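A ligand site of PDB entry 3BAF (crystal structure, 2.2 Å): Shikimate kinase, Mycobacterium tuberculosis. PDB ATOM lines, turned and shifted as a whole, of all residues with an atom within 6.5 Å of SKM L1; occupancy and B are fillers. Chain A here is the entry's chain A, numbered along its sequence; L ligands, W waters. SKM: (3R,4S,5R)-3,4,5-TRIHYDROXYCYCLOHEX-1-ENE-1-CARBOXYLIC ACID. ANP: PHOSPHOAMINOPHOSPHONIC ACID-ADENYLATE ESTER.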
ATOM      1  N   LEU A  10     -11.371 -13.056 -27.349  1.00  0.00           N
ATOM      2  CA  LEU A  10     -10.906 -14.516 -27.308  1.00  0.00           C
ATOM      3  C   LEU A  10      -9.839 -14.779 -26.229  1.00  0.00           C
ATOM      4  O   LEU A  10      -9.105 -13.836 -25.866  1.00  0.00           O
ATOM      5  CB  LEU A  10     -10.297 -14.980 -28.689  1.00  0.00           C
ATOM      6  CG  LEU A  10     -11.146 -14.994 -30.021  1.00  0.00           C
ATOM      7  CD1 LEU A  10     -10.320 -15.049 -31.341  1.00  0.00           C
ATOM      8  CD2 LEU A  10     -12.272 -16.128 -30.054  1.00  0.00           C
ATOM      9  N   PRO A  11      -9.700 -16.039 -25.762  1.00  0.00           N
ATOM     10  CA  PRO A  11      -8.550 -16.449 -24.907  1.00  0.00           C
ATOM     11  C   PRO A  11      -7.181 -16.053 -25.520  1.00  0.00           C
ATOM     12  O   PRO A  11      -7.012 -16.196 -26.750  1.00  0.00           O
ATOM     13  CB  PRO A  11      -8.726 -17.984 -24.753  1.00  0.00           C
ATOM     14  CG  PRO A  11      -9.695 -18.359 -25.852  1.00  0.00           C
ATOM     15  CD  PRO A  11     -10.606 -17.174 -26.036  1.00  0.00           C
ATOM     16  N   LYS A  15      -7.189  -9.782 -21.730  1.00  0.00           N
ATOM     17  CA  LYS A  15      -8.198  -9.339 -20.664  1.00  0.00           C
ATOM     18  C   LYS A  15      -7.631  -9.281 -19.185  1.00  0.00           C
ATOM     19  O   LYS A  15      -7.805  -8.246 -18.507  1.00  0.00           O
ATOM     20  CB  LYS A  15      -9.519 -10.192 -20.698  1.00  0.00           C
ATOM     21  CG  LYS A  15     -10.363 -10.183 -22.039  1.00  0.00           C
ATOM     22  CD  LYS A  15     -11.632 -11.202 -22.128  1.00  0.00           C
ATOM     23  CE  LYS A  15     -11.405 -12.746 -21.751  1.00  0.00           C
ATOM     24  NZ  LYS A  15     -10.552 -13.514 -22.822  1.00  0.00           N
ATOM     25  N   ASP A  34     -14.157 -14.905 -13.752  1.00  0.00           N
ATOM     26  CA  ASP A  34     -13.726 -16.351 -13.598  1.00  0.00           C
ATOM     27  C   ASP A  34     -13.255 -16.701 -12.192  1.00  0.00           C
ATOM     28  O   ASP A  34     -13.565 -17.787 -11.709  1.00  0.00           O
ATOM     29  CB  ASP A  34     -12.568 -16.799 -14.559  1.00  0.00           C
ATOM     30  CG  ASP A  34     -12.938 -16.857 -16.065  1.00  0.00           C
ATOM     31  OD1 ASP A  34     -14.094 -17.255 -16.392  1.00  0.00           O
ATOM     32  OD2 ASP A  34     -12.065 -16.523 -16.922  1.00  0.00           O
ATOM     33  N   ILE A  45     -12.991 -24.543 -12.578  1.00  0.00           N
ATOM     34  CA  ILE A  45     -13.769 -24.404 -13.834  1.00  0.00           C
ATOM     35  C   ILE A  45     -13.814 -25.739 -14.591  1.00  0.00           C
ATOM     36  O   ILE A  45     -14.867 -26.125 -15.098  1.00  0.00           O
ATOM     37  CB  ILE A  45     -13.216 -23.286 -14.798  1.00  0.00           C
ATOM     38  CG1 ILE A  45     -12.942 -21.970 -14.064  1.00  0.00           C
ATOM     39  CG2 ILE A  45     -14.108 -23.124 -16.020  1.00  0.00           C
ATOM     40  CD1 ILE A  45     -14.108 -21.059 -13.871  1.00  0.00           C
ATOM     41  N   PHE A  49     -17.421 -28.070 -15.571  1.00  0.00           N
ATOM     42  CA  PHE A  49     -17.570 -28.566 -16.957  1.00  0.00           C
ATOM     43  C   PHE A  49     -17.696 -30.115 -16.990  1.00  0.00           C
ATOM     44  O   PHE A  49     -18.579 -30.636 -17.698  1.00  0.00           O
ATOM     45  CB  PHE A  49     -16.433 -28.035 -17.884  1.00  0.00           C
ATOM     46  CG  PHE A  49     -16.775 -26.746 -18.670  1.00  0.00           C
ATOM     47  CD1 PHE A  49     -17.152 -26.799 -20.006  1.00  0.00           C
ATOM     48  CD2 PHE A  49     -16.690 -25.481 -18.072  1.00  0.00           C
ATOM     49  CE1 PHE A  49     -17.474 -25.623 -20.747  1.00  0.00           C
ATOM     50  CE2 PHE A  49     -16.991 -24.293 -18.784  1.00  0.00           C
ATOM     51  CZ  PHE A  49     -17.397 -24.372 -20.134  1.00  0.00           C
ATOM     52  N   GLU A  54     -21.507 -27.520 -19.759  1.00  0.00           N
ATOM     53  CA  GLU A  54     -21.459 -26.086 -20.189  1.00  0.00           C
ATOM     54  C   GLU A  54     -22.747 -25.243 -19.985  1.00  0.00           C
ATOM     55  O   GLU A  54     -22.672 -24.066 -19.610  1.00  0.00           O
ATOM     56  CB  GLU A  54     -20.938 -25.927 -21.657  1.00  0.00           C
ATOM     57  CG  GLU A  54     -21.306 -24.593 -22.396  1.00  0.00           C
ATOM     58  CD  GLU A  54     -20.610 -24.342 -23.767  1.00  0.00           C
ATOM     59  OE1 GLU A  54     -20.672 -23.186 -24.254  1.00  0.00           O
ATOM     60  OE2 GLU A  54     -20.043 -25.276 -24.408  1.00  0.00           O
ATOM     61  N   PHE A  57     -22.709 -24.181 -16.327  1.00  0.00           N
ATOM     62  CA  PHE A  57     -21.717 -23.066 -16.233  1.00  0.00           C
ATOM     63  C   PHE A  57     -22.298 -21.692 -16.660  1.00  0.00           C
ATOM     64  O   PHE A  57     -22.147 -20.707 -15.907  1.00  0.00           O
ATOM     65  CB  PHE A  57     -20.356 -23.379 -16.958  1.00  0.00           C
ATOM     66  CG  PHE A  57     -19.334 -22.212 -16.913  1.00  0.00           C
ATOM     67  CD1 PHE A  57     -18.506 -22.025 -15.814  1.00  0.00           C
ATOM     68  CD2 PHE A  57     -19.228 -21.302 -17.973  1.00  0.00           C
ATOM     69  CE1 PHE A  57     -17.582 -20.934 -15.754  1.00  0.00           C
ATOM     70  CE2 PHE A  57     -18.292 -20.260 -17.963  1.00  0.00           C
ATOM     71  CZ  PHE A  57     -17.480 -20.056 -16.841  1.00  0.00           C
ATOM     72  N   ARG A  58     -22.972 -21.636 -17.804  1.00  0.00           N
ATOM     73  CA  ARG A  58     -23.550 -20.379 -18.349  1.00  0.00           C
ATOM     74  C   ARG A  58     -24.632 -19.700 -17.468  1.00  0.00           C
ATOM     75  O   ARG A  58     -24.708 -18.458 -17.416  1.00  0.00           O
ATOM     76  CB  ARG A  58     -24.112 -20.560 -19.775  1.00  0.00           C
ATOM     77  CG  ARG A  58     -23.123 -21.021 -20.829  1.00  0.00           C
ATOM     78  CD  ARG A  58     -22.008 -19.998 -21.236  1.00  0.00           C
ATOM     79  NE  ARG A  58     -20.951 -20.628 -22.041  1.00  0.00           N
ATOM     80  CZ  ARG A  58     -19.668 -20.238 -22.134  1.00  0.00           C
ATOM     81  NH1 ARG A  58     -19.208 -19.158 -21.471  1.00  0.00           N
ATOM     82  NH2 ARG A  58     -18.821 -20.962 -22.870  1.00  0.00           N
ATOM     83  N   GLU A  61     -22.692 -17.984 -14.430  1.00  0.00           N
ATOM     84  CA  GLU A  61     -21.972 -16.839 -15.029  1.00  0.00           C
ATOM     85  C   GLU A  61     -22.889 -15.577 -15.260  1.00  0.00           C
ATOM     86  O   GLU A  61     -22.524 -14.463 -14.843  1.00  0.00           O
ATOM     87  CB  GLU A  61     -21.188 -17.302 -16.299  1.00  0.00           C
ATOM     88  CG  GLU A  61     -20.321 -16.227 -17.073  1.00  0.00           C
ATOM     89  CD  GLU A  61     -19.639 -16.746 -18.404  1.00  0.00           C
ATOM     90  OE1 GLU A  61     -20.346 -17.250 -19.330  1.00  0.00           O
ATOM     91  OE2 GLU A  61     -18.385 -16.572 -18.543  1.00  0.00           O
ATOM     92  N   LEU A  78     -14.413  -9.844 -18.142  1.00  0.00           N
ATOM     93  CA  LEU A  78     -15.366 -10.977 -18.472  1.00  0.00           C
ATOM     94  C   LEU A  78     -14.735 -12.346 -18.987  1.00  0.00           C
ATOM     95  O   LEU A  78     -13.751 -12.311 -19.712  1.00  0.00           O
ATOM     96  CB  LEU A  78     -16.387 -10.447 -19.527  1.00  0.00           C
ATOM     97  CG  LEU A  78     -17.756  -9.851 -19.128  1.00  0.00           C
ATOM     98  CD1 LEU A  78     -17.719  -8.931 -17.812  1.00  0.00           C
ATOM     99  CD2 LEU A  78     -18.712  -9.327 -20.276  1.00  0.00           C
ATOM    100  N   GLY A  79     -15.235 -13.530 -18.633  1.00  0.00           N
ATOM    101  CA  GLY A  79     -14.846 -14.784 -19.359  1.00  0.00           C
ATOM    102  C   GLY A  79     -14.992 -14.789 -20.894  1.00  0.00           C
ATOM    103  O   GLY A  79     -15.820 -14.051 -21.447  1.00  0.00           O
ATOM    104  N   GLY A  80     -14.199 -15.579 -21.624  1.00  0.00           N
ATOM    105  CA  GLY A  80     -14.205 -15.486 -23.116  1.00  0.00           C
ATOM    106  C   GLY A  80     -15.474 -15.788 -23.933  1.00  0.00           C
ATOM    107  O   GLY A  80     -15.678 -15.224 -25.023  1.00  0.00           O
ATOM    108  N   GLY A  81     -16.345 -16.676 -23.418  1.00  0.00           N
ATOM    109  CA  GLY A  81     -17.604 -17.007 -24.083  1.00  0.00           C
ATOM    110  C   GLY A  81     -18.875 -16.385 -23.444  1.00  0.00           C
ATOM    111  O   GLY A  81     -20.029 -16.818 -23.745  1.00  0.00           O
ATOM    112  N   ALA A  82     -18.687 -15.371 -22.580  1.00  0.00           N
ATOM    113  CA  ALA A  82     -19.874 -14.706 -21.956  1.00  0.00           C
ATOM    114  C   ALA A  82     -20.823 -14.017 -22.974  1.00  0.00           C
ATOM    115  O   ALA A  82     -22.039 -14.004 -22.767  1.00  0.00           O
ATOM    116  CB  ALA A  82     -19.463 -13.714 -20.805  1.00  0.00           C
ATOM    117  N   ARG A 117      -8.024 -24.903 -20.113  1.00  0.00           N
ATOM    118  CA  ARG A 117      -9.098 -24.506 -21.032  1.00  0.00           C
ATOM    119  C   ARG A 117      -9.895 -25.657 -21.743  1.00  0.00           C
ATOM    120  O   ARG A 117      -9.601 -25.988 -22.903  1.00  0.00           O
ATOM    121  CB  ARG A 117      -8.624 -23.369 -21.957  1.00  0.00           C
ATOM    122  CG  ARG A 117      -8.231 -22.079 -21.203  1.00  0.00           C
ATOM    123  CD  ARG A 117      -7.876 -20.964 -22.170  1.00  0.00           C
ATOM    124  NE  ARG A 117      -7.390 -19.689 -21.600  1.00  0.00           N
ATOM    125  CZ  ARG A 117      -6.106 -19.313 -21.482  1.00  0.00           C
ATOM    126  NH1 ARG A 117      -5.101 -20.128 -21.796  1.00  0.00           N
ATOM    127  NH2 ARG A 117      -5.810 -18.123 -20.975  1.00  0.00           N
ATOM    128  N   PRO A 118     -10.931 -26.218 -21.059  1.00  0.00           N
ATOM    129  CA  PRO A 118     -11.815 -27.284 -21.570  1.00  0.00           C
ATOM    130  C   PRO A 118     -12.194 -27.226 -23.072  1.00  0.00           C
ATOM    131  O   PRO A 118     -12.355 -28.297 -23.694  1.00  0.00           O
ATOM    132  CB  PRO A 118     -13.093 -27.145 -20.729  1.00  0.00           C
ATOM    133  CG  PRO A 118     -12.718 -26.396 -19.498  1.00  0.00           C
ATOM    134  CD  PRO A 118     -11.311 -25.828 -19.684  1.00  0.00           C
ATOM    135  N   LEU A 119     -12.339 -26.035 -23.654  1.00  0.00           N
ATOM    136  CA  LEU A 119     -12.797 -25.898 -25.026  1.00  0.00           C
ATOM    137  C   LEU A 119     -11.682 -25.875 -26.117  1.00  0.00           C
ATOM    138  O   LEU A 119     -11.980 -25.962 -27.312  1.00  0.00           O
ATOM    139  CB  LEU A 119     -13.817 -24.739 -25.163  1.00  0.00           C
ATOM    140  CG  LEU A 119     -15.336 -24.912 -25.370  1.00  0.00           C
ATOM    141  CD1 LEU A 119     -15.990 -26.160 -24.781  1.00  0.00           C
ATOM    142  CD2 LEU A 119     -16.095 -23.685 -24.889  1.00  0.00           C
ATOM    143  N   LEU A 132     -13.773 -21.375 -33.356  1.00  0.00           N
ATOM    144  CA  LEU A 132     -14.179 -20.326 -32.360  1.00  0.00           C
ATOM    145  C   LEU A 132     -14.151 -18.829 -32.858  1.00  0.00           C
ATOM    146  O   LEU A 132     -15.095 -18.057 -32.579  1.00  0.00           O
ATOM    147  CB  LEU A 132     -13.234 -20.489 -31.145  1.00  0.00           C
ATOM    148  CG  LEU A 132     -13.735 -21.004 -29.794  1.00  0.00           C
ATOM    149  CD1 LEU A 132     -14.547 -22.257 -29.951  1.00  0.00           C
ATOM    150  CD2 LEU A 132     -12.618 -21.081 -28.704  1.00  0.00           C
ATOM    151  N   ARG A 136     -17.708 -16.416 -33.139  1.00  0.00           N
ATOM    152  CA  ARG A 136     -17.845 -15.286 -32.202  1.00  0.00           C
ATOM    153  C   ARG A 136     -17.634 -13.846 -32.713  1.00  0.00           C
ATOM    154  O   ARG A 136     -18.140 -12.888 -32.106  1.00  0.00           O
ATOM    155  CB  ARG A 136     -17.124 -15.515 -30.877  1.00  0.00           C
ATOM    156  CG  ARG A 136     -16.930 -16.990 -30.405  1.00  0.00           C
ATOM    157  CD  ARG A 136     -17.538 -17.403 -29.093  1.00  0.00           C
ATOM    158  NE  ARG A 136     -16.711 -18.273 -28.235  1.00  0.00           N
ATOM    159  CZ  ARG A 136     -17.221 -19.144 -27.355  1.00  0.00           C
ATOM    160  NH1 ARG A 136     -18.537 -19.245 -27.297  1.00  0.00           N
ATOM    161  NH2 ARG A 136     -16.516 -19.973 -26.552  1.00  0.00           N
ATOM    162  N   TYR A 140     -18.798  -9.996 -30.703  1.00  0.00           N
ATOM    163  CA  TYR A 140     -17.878  -8.901 -30.212  1.00  0.00           C
ATOM    164  C   TYR A 140     -18.140  -7.531 -30.962  1.00  0.00           C
ATOM    165  O   TYR A 140     -18.216  -6.460 -30.332  1.00  0.00           O
ATOM    166  CB  TYR A 140     -16.363  -9.295 -30.302  1.00  0.00           C
ATOM    167  CG  TYR A 140     -15.909 -10.593 -29.584  1.00  0.00           C
ATOM    168  CD1 TYR A 140     -16.130 -10.781 -28.257  1.00  0.00           C
ATOM    169  CD2 TYR A 140     -15.298 -11.644 -30.293  1.00  0.00           C
ATOM    170  CE1 TYR A 140     -15.758 -11.984 -27.592  1.00  0.00           C
ATOM    171  CE2 TYR A 140     -14.858 -12.827 -29.655  1.00  0.00           C
ATOM    172  CZ  TYR A 140     -15.083 -12.988 -28.297  1.00  0.00           C
ATOM    173  OH  TYR A 140     -14.705 -14.166 -27.610  1.00  0.00           O
HETATM  174  O12 SKM L   1     -14.359 -18.697 -18.869  1.00  0.00           O
HETATM  175  C8  SKM L   1     -13.266 -19.487 -19.418  1.00  0.00           C
HETATM  176  C6  SKM L   1     -12.352 -18.852 -20.536  1.00  0.00           C
HETATM  177  O7  SKM L   1     -11.991 -17.418 -20.358  1.00  0.00           O
HETATM  178  C5  SKM L   1     -12.769 -19.303 -21.981  1.00  0.00           C
HETATM  179  C4  SKM L   1     -13.983 -19.871 -22.260  1.00  0.00           C
HETATM  180  C1  SKM L   1     -14.554 -19.842 -23.488  1.00  0.00           C
HETATM  181  O2  SKM L   1     -15.755 -20.314 -23.601  1.00  0.00           O
HETATM  182  O3  SKM L   1     -13.935 -19.346 -24.505  1.00  0.00           O
HETATM  183  C10 SKM L   1     -14.672 -20.429 -21.232  1.00  0.00           C
HETATM  184  C9  SKM L   1     -13.920 -20.784 -19.939  1.00  0.00           C
HETATM  185  O11 SKM L   1     -12.930 -21.851 -20.023  1.00  0.00           O
HETATM  186  PG  ANP L   2      -9.487 -16.312 -20.799  1.00  0.00           P
HETATM  187  O1G ANP L   2      -9.335 -17.734 -20.246  1.00  0.00           O
HETATM  188  O2G ANP L   2     -10.296 -15.709 -19.643  1.00  0.00           O
HETATM  189  O3G ANP L   2     -10.402 -16.392 -21.968  1.00  0.00           O
HETATM  190  PB  ANP L   2      -6.975 -13.745 -21.398  1.00  0.00           P
HETATM  191  O1B ANP L   2      -7.595 -12.918 -22.533  1.00  0.00           O
HETATM  192  O2B ANP L   2      -7.328 -13.099 -20.073  1.00  0.00           O
HETATM  193  N3B ANP L   2      -7.732 -15.465 -21.215  1.00  0.00           N
HETATM  194  PA  ANP L   2      -4.075 -13.019 -20.610  1.00  0.00           P
HETATM  195  O1A ANP L   2      -4.043 -11.649 -19.998  1.00  0.00           O
HETATM  196  O2A ANP L   2      -4.059 -14.201 -19.738  1.00  0.00           O
HETATM  197  O3A ANP L   2      -5.377 -13.213 -21.652  1.00  0.00           O
HETATM  198  O5' ANP L   2      -2.712 -13.154 -21.546  1.00  0.00           O
HETATM  199  C5' ANP L   2      -2.146 -14.420 -22.050  1.00  0.00           C
HETATM  200  C4' ANP L   2      -0.586 -14.401 -22.177  1.00  0.00           C
HETATM  201  O4' ANP L   2      -0.264 -13.499 -23.244  1.00  0.00           O
HETATM  202  C3' ANP L   2       0.144 -13.883 -20.884  1.00  0.00           C
HETATM  203  O3' ANP L   2       1.388 -14.536 -20.427  1.00  0.00           O
HETATM  204  C2' ANP L   2       0.487 -12.460 -21.237  1.00  0.00           C
HETATM  205  O2' ANP L   2       1.713 -12.184 -20.537  1.00  0.00           O
HETATM  206  C1' ANP L   2       0.611 -12.417 -22.774  1.00  0.00           C
HETATM  207  N9  ANP L   2       0.310 -11.103 -23.426  1.00  0.00           N
HETATM  208  C8  ANP L   2      -0.918 -10.446 -23.265  1.00  0.00           C
HETATM  209  N7  ANP L   2      -0.988  -9.292 -23.996  1.00  0.00           N
HETATM  210  C5  ANP L   2       0.197  -9.173 -24.668  1.00  0.00           C
HETATM  211  C6  ANP L   2       0.800  -8.166 -25.558  1.00  0.00           C
HETATM  212  N6  ANP L   2       0.139  -7.029 -25.948  1.00  0.00           N
HETATM  213  N1  ANP L   2       2.076  -8.405 -26.020  1.00  0.00           N
HETATM  214  C2  ANP L   2       2.810  -9.498 -25.635  1.00  0.00           C
HETATM  215  N3  ANP L   2       2.323 -10.458 -24.848  1.00  0.00           N
HETATM  216  C4  ANP L   2       1.052 -10.358 -24.281  1.00  0.00           C
HETATM  217  O   HOH W   1     -10.500 -21.828 -18.033  1.00  0.00           O
HETATM  218  O   HOH W   2     -12.192 -23.103 -22.478  1.00  0.00           O
HETATM  219  O   HOH W   3     -11.504 -21.498 -24.500  1.00  0.00           O
HETATM  220  O   HOH W   4     -16.500 -17.881 -20.455  1.00  0.00           O
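An oxygen (O3G) of ANP L2 sits at hydrogen-bond distance from an oxygen (O7) of SKM L1 (2.5 Å).
The guanidinium group (NH2) of Arg 58 lies within salt-bridge range of an oxygen (O2) of SKM L1 (3.2 Å).
NH2 of Arg 136 is in salt-bridge range of O2 of SKM L1 (3.1 Å).
An oxygen (O1G) of ANP L2 lies within salt-bridge range of the guanidinium group (NE) of Arg 117, at 3.1 Å.
OD1 of Asp 34 sits at hydrogen-bond distance from O12 of SKM L1 (2.9 Å).
NZ of Lys 15 is in salt-bridge range of O3G of ANP L2, 3.0 Å away.
An oxygen (O7) of SKM L1 is in hydrogen-bond range of the backbone NH of Gly 80 (3.1 Å).
The backbone NH (N) of Lys 15 sits at hydrogen-bond distance from an oxygen (O1B) of ANP L2 (3.3 Å).
The backbone carbonyl oxygen of Gly 81 lies within hydrogen-bond range of the guanidinium group of Arg 58 (3.4 Å).
The guanidinium group (NH1) of Arg 58 lies within salt-bridge range of the side-chain carboxylate (OE1) of Glu 61, at 3.1 Å.
O of Gly 80 is in hydrogen-bond range of OH of Tyr 140 (3.0 Å).
NH2 of Arg 58 lies within salt-bridge range of OE1 of Glu 54, 3.2 Å away.
Water W2 bridges an oxygen (O11) of SKM L1 (2.9 Å) and the backbone NH (N) of Leu 119 (3.2 Å).
Phe 57 touches SKM L1 (CZ to O12, 3.96 Å).
Gly 79 touches SKM L1 (CA to O12, 3.97 Å).
N of Gly 81 touches C1 of SKM L1 (3.6 Å).
CD2 of Leu 119 touches O2 of SKM L1, 3.6 Å away.
Hydrophobic or aromatic side chains within 4 Å of SKM L1: Phe 57 and Leu 119.
Of the 21 residues printed, 8 come within 4 Å of SKM L1.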
